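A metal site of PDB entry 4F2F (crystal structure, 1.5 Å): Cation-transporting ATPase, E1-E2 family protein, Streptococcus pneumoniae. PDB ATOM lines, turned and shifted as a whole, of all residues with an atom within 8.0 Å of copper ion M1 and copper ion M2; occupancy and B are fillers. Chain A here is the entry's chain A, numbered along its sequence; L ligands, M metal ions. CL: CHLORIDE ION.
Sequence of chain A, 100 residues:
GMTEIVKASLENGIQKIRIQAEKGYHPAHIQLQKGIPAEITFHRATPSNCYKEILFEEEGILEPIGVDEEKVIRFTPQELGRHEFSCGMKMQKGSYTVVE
Within 4 Å of copper ion M2: Cys 50, Cys 87, Met 89 and Met 91.
The nearest printed residue that does not touch copper ion M2 is Gln 92 (4.1 Å).
The side-chain sulfur (SG) of Cys 87 lies close to the backbone NH (N) of Met 91.
N of Met 89 lies close to SG of Cys 87 (3.4 Å).
The backbone carbonyl oxygen (O) of Gln 92 is in hydrogen-bond range of the backbone NH (N) of Cys 87, 3.0 Å away.
SG of Cys 87 lies close to N of Lys 90 (3.5 Å).
The backbone NH (N) of Cys 87 lies close to the side-chain hydroxyl (OH) of Tyr 25 (3.3 Å).
The backbone NH (N) of Cys 50 lies close to the side-chain hydroxyl (OG) of Ser 48 (3.2 Å).
Within 4 Å of copper ion M1: Cys 50, Met 89 and Met 91.
Along chain A the residues within 4 Å of copper ion M1 span positions 50 to 91.
Copper ion M1 is bound by the side-chain sulfur (SG) of Cys 50.
The side-chain sulfur (SD) of Met 91 binds copper ion M1.
Copper ion M1 is bound by SD of Met 89, at 2.3 Å.
CL of the ligand is bound to copper ion M1.
Copper ion M2 is bound by SG of Cys 87, SG of Cys 50 and O of Cys 50.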
ATOM      1  N   TYR A  25     -24.030  15.674  26.615  1.00  0.00           N
ATOM      2  CA  TYR A  25     -22.628  15.322  26.790  1.00  0.00           C
ATOM      3  C   TYR A  25     -21.861  16.491  27.381  1.00  0.00           C
ATOM      4  O   TYR A  25     -22.108  17.647  27.017  1.00  0.00           O
ATOM      5  CB  TYR A  25     -22.017  14.891  25.455  1.00  0.00           C
ATOM      6  CG  TYR A  25     -22.583  13.614  24.901  1.00  0.00           C
ATOM      7  CD1 TYR A  25     -22.261  12.381  25.452  1.00  0.00           C
ATOM      8  CD2 TYR A  25     -23.464  13.626  23.827  1.00  0.00           C
ATOM      9  CE1 TYR A  25     -22.784  11.209  24.949  1.00  0.00           C
ATOM     10  CE2 TYR A  25     -23.988  12.456  23.314  1.00  0.00           C
ATOM     11  CZ  TYR A  25     -23.647  11.247  23.880  1.00  0.00           C
ATOM     12  OH  TYR A  25     -24.180  10.078  23.377  1.00  0.00           O
ATOM     13  N   SER A  48     -30.988   6.301  31.086  1.00  0.00           N
ATOM     14  CA  SER A  48     -31.743   6.507  29.854  1.00  0.00           C
ATOM     15  C   SER A  48     -31.088   5.824  28.663  1.00  0.00           C
ATOM     16  O   SER A  48     -29.913   6.045  28.392  1.00  0.00           O
ATOM     17  CB  SER A  48     -31.905   7.998  29.544  1.00  0.00           C
ATOM     18  OG  SER A  48     -32.486   8.174  28.263  1.00  0.00           O
ATOM     19  N   ASN A  49     -31.858   5.019  27.939  1.00  0.00           N
ATOM     20  CA  ASN A  49     -31.321   4.356  26.763  1.00  0.00           C
ATOM     21  C   ASN A  49     -31.094   5.289  25.565  1.00  0.00           C
ATOM     22  O   ASN A  49     -30.596   4.866  24.528  1.00  0.00           O
ATOM     23  CB  ASN A  49     -32.168   3.157  26.341  1.00  0.00           C
ATOM     24  CG  ASN A  49     -31.671   1.863  26.949  1.00  0.00           C
ATOM     25  OD1 ASN A  49     -30.611   1.822  27.567  1.00  0.00           O
ATOM     26  ND2 ASN A  49     -32.444   0.796  26.776  1.00  0.00           N
ATOM     27  N   CYS A  50     -31.430   6.562  25.724  1.00  0.00           N
ATOM     28  CA  CYS A  50     -31.097   7.538  24.696  1.00  0.00           C
ATOM     29  C   CYS A  50     -29.581   7.579  24.517  1.00  0.00           C
ATOM     30  O   CYS A  50     -29.073   7.949  23.460  1.00  0.00           O
ATOM     31  CB  CYS A  50     -31.636   8.924  25.064  1.00  0.00           C
ATOM     32  SG  CYS A  50     -31.577  10.153  23.731  1.00  0.00           S
ATOM     33  N   TYR A  51     -28.864   7.166  25.557  1.00  0.00           N
ATOM     34  CA  TYR A  51     -27.404   7.216  25.584  1.00  0.00           C
ATOM     35  C   TYR A  51     -26.749   5.837  25.501  1.00  0.00           C
ATOM     36  O   TYR A  51     -25.578   5.694  25.873  1.00  0.00           O
ATOM     37  CB  TYR A  51     -26.920   7.937  26.857  1.00  0.00           C
ATOM     38  CG  TYR A  51     -27.437   9.346  27.015  1.00  0.00           C
ATOM     39  CD1 TYR A  51     -26.678  10.428  26.621  1.00  0.00           C
ATOM     40  CD2 TYR A  51     -28.695   9.582  27.569  1.00  0.00           C
ATOM     41  CE1 TYR A  51     -27.153  11.721  26.776  1.00  0.00           C
ATOM     42  CE2 TYR A  51     -29.174  10.863  27.732  1.00  0.00           C
ATOM     43  CZ  TYR A  51     -28.398  11.933  27.326  1.00  0.00           C
ATOM     44  OH  TYR A  51     -28.877  13.216  27.479  1.00  0.00           O
ATOM     45  N   LYS A  52     -27.473   4.835  25.024  1.00  0.00           N
ATOM     46  CA  LYS A  52     -26.945   3.468  25.016  1.00  0.00           C
ATOM     47  C   LYS A  52     -25.902   3.224  23.934  1.00  0.00           C
ATOM     48  O   LYS A  52     -25.244   2.179  23.926  1.00  0.00           O
ATOM     49  CB  LYS A  52     -28.068   2.438  24.906  1.00  0.00           C
ATOM     50  CG  LYS A  52     -28.671   2.293  23.512  1.00  0.00           C
ATOM     51  CD  LYS A  52     -29.714   1.191  23.489  1.00  0.00           C
ATOM     52  CE  LYS A  52     -30.148   0.877  22.060  1.00  0.00           C
ATOM     53  NZ  LYS A  52     -31.140  -0.227  22.025  1.00  0.00           N
ATOM     54  N   GLU A  53     -25.744   4.175  23.025  1.00  0.00           N
ATOM     55  CA  GLU A  53     -24.758   4.060  21.959  1.00  0.00           C
ATOM     56  C   GLU A  53     -24.018   5.373  21.722  1.00  0.00           C
ATOM     57  O   GLU A  53     -24.534   6.452  22.000  1.00  0.00           O
ATOM     58  CB  GLU A  53     -25.417   3.575  20.663  1.00  0.00           C
ATOM     59  CG  GLU A  53     -25.827   2.110  20.703  1.00  0.00           C
ATOM     60  CD  GLU A  53     -26.935   1.768  19.717  1.00  0.00           C
ATOM     61  OE1 GLU A  53     -27.334   2.665  18.939  1.00  0.00           O
ATOM     62  OE2 GLU A  53     -27.398   0.610  19.724  1.00  0.00           O
ATOM     63  N   SER A  86     -22.504  11.953  18.335  1.00  0.00           N
ATOM     64  CA  SER A  86     -23.805  11.975  18.971  1.00  0.00           C
ATOM     65  C   SER A  86     -24.085  10.642  19.624  1.00  0.00           C
ATOM     66  O   SER A  86     -23.272   9.725  19.546  1.00  0.00           O
ATOM     67  CB  SER A  86     -24.896  12.273  17.935  1.00  0.00           C
ATOM     68  OG  SER A  86     -25.080  11.181  17.055  1.00  0.00           O
ATOM     69  N   CYS A  87     -25.232  10.539  20.295  1.00  0.00           N
ATOM     70  CA  CYS A  87     -25.717   9.234  20.722  1.00  0.00           C
ATOM     71  C   CYS A  87     -26.179   8.468  19.492  1.00  0.00           C
ATOM     72  O   CYS A  87     -26.211   9.003  18.383  1.00  0.00           O
ATOM     73  CB  CYS A  87     -26.874   9.392  21.708  1.00  0.00           C
ATOM     74  SG  CYS A  87     -28.365  10.086  20.979  1.00  0.00           S
ATOM     75  N   GLY A  88     -26.534   7.200  19.690  1.00  0.00           N
ATOM     76  CA  GLY A  88     -26.986   6.364  18.588  1.00  0.00           C
ATOM     77  C   GLY A  88     -28.306   6.814  17.993  1.00  0.00           C
ATOM     78  O   GLY A  88     -28.668   6.375  16.895  1.00  0.00           O
ATOM     79  N   MET A  89     -29.030   7.674  18.690  1.00  0.00           N
ATOM     80  CA  MET A  89     -30.325   8.148  18.211  1.00  0.00           C
ATOM     81  C   MET A  89     -30.185   9.481  17.488  1.00  0.00           C
ATOM     82  O   MET A  89     -31.147   9.986  16.898  1.00  0.00           O
ATOM     83  CB  MET A  89     -31.319   8.292  19.354  1.00  0.00           C
ATOM     84  CG  MET A  89     -31.516   7.027  20.193  1.00  0.00           C
ATOM     85  SD  MET A  89     -32.832   7.230  21.404  1.00  0.00           S
ATOM     86  CE  MET A  89     -34.287   6.874  20.410  1.00  0.00           C
ATOM     87  N   LYS A  90     -28.984  10.052  17.560  1.00  0.00           N
ATOM     88  CA  LYS A  90     -28.709  11.378  17.007  1.00  0.00           C
ATOM     89  C   LYS A  90     -29.558  12.473  17.659  1.00  0.00           C
ATOM     90  O   LYS A  90     -29.775  13.534  17.073  1.00  0.00           O
ATOM     91  CB  LYS A  90     -28.848  11.368  15.479  1.00  0.00           C
ATOM     92  CG  LYS A  90     -27.834  10.466  14.790  1.00  0.00           C
ATOM     93  CD  LYS A  90     -28.200  10.135  13.346  1.00  0.00           C
ATOM     94  CE  LYS A  90     -28.055  11.344  12.437  1.00  0.00           C
ATOM     95  NZ  LYS A  90     -28.198  10.958  11.000  1.00  0.00           N
ATOM     96  N   MET A  91     -30.013  12.213  18.890  1.00  0.00           N
ATOM     97  CA  MET A  91     -30.796  13.183  19.649  1.00  0.00           C
ATOM     98  C   MET A  91     -29.906  14.088  20.503  1.00  0.00           C
ATOM     99  O   MET A  91     -30.153  15.278  20.625  1.00  0.00           O
ATOM    100  CB  MET A  91     -31.820  12.486  20.539  1.00  0.00           C
ATOM    101  CG  MET A  91     -32.900  11.734  19.779  1.00  0.00           C
ATOM    102  SD  MET A  91     -34.021  10.828  20.854  1.00  0.00           S
ATOM    103  CE  MET A  91     -34.942  12.164  21.626  1.00  0.00           C
ATOM    104  N   GLN A  92     -28.874  13.499  21.096  1.00  0.00           N
ATOM    105  CA  GLN A  92     -27.907  14.245  21.887  1.00  0.00           C
ATOM    106  C   GLN A  92     -26.612  14.391  21.101  1.00  0.00           C
ATOM    107  O   GLN A  92     -25.996  13.396  20.726  1.00  0.00           O
ATOM    108  CB  GLN A  92     -27.653  13.550  23.226  1.00  0.00           C
ATOM    109  CG  GLN A  92     -28.898  13.416  24.096  1.00  0.00           C
ATOM    110  CD  GLN A  92     -29.400  14.756  24.597  1.00  0.00           C
ATOM    111  OE1 GLN A  92     -28.641  15.714  24.698  1.00  0.00           O
ATOM    112  NE2 GLN A  92     -30.690  14.826  24.905  1.00  0.00           N
ATOM    113  N   LYS A  93     -26.204  15.633  20.846  1.00  0.00           N
ATOM    114  CA  LYS A  93     -25.085  15.882  19.949  1.00  0.00           C
ATOM    115  C   LYS A  93     -23.890  16.590  20.597  1.00  0.00           C
ATOM    116  O   LYS A  93     -24.001  17.203  21.664  1.00  0.00           O
ATOM    117  CB  LYS A  93     -25.541  16.715  18.752  1.00  0.00           C
ATOM    118  CG  LYS A  93     -26.620  16.062  17.920  1.00  0.00           C
ATOM    119  CD  LYS A  93     -27.184  17.058  16.919  1.00  0.00           C
ATOM    120  CE  LYS A  93     -28.230  16.427  16.029  1.00  0.00           C
ATOM    121  NZ  LYS A  93     -28.930  17.448  15.219  1.00  0.00           N
HETATM  122 CL    CL L   1     -34.855   8.663  23.739  1.00  0.00          CL
HETATM  123 CU    CU M   1     -33.028   9.372  22.238  1.00  0.00          CU
HETATM  124 CU    CU M   2     -29.829   9.782  22.522  1.00  0.00          CU
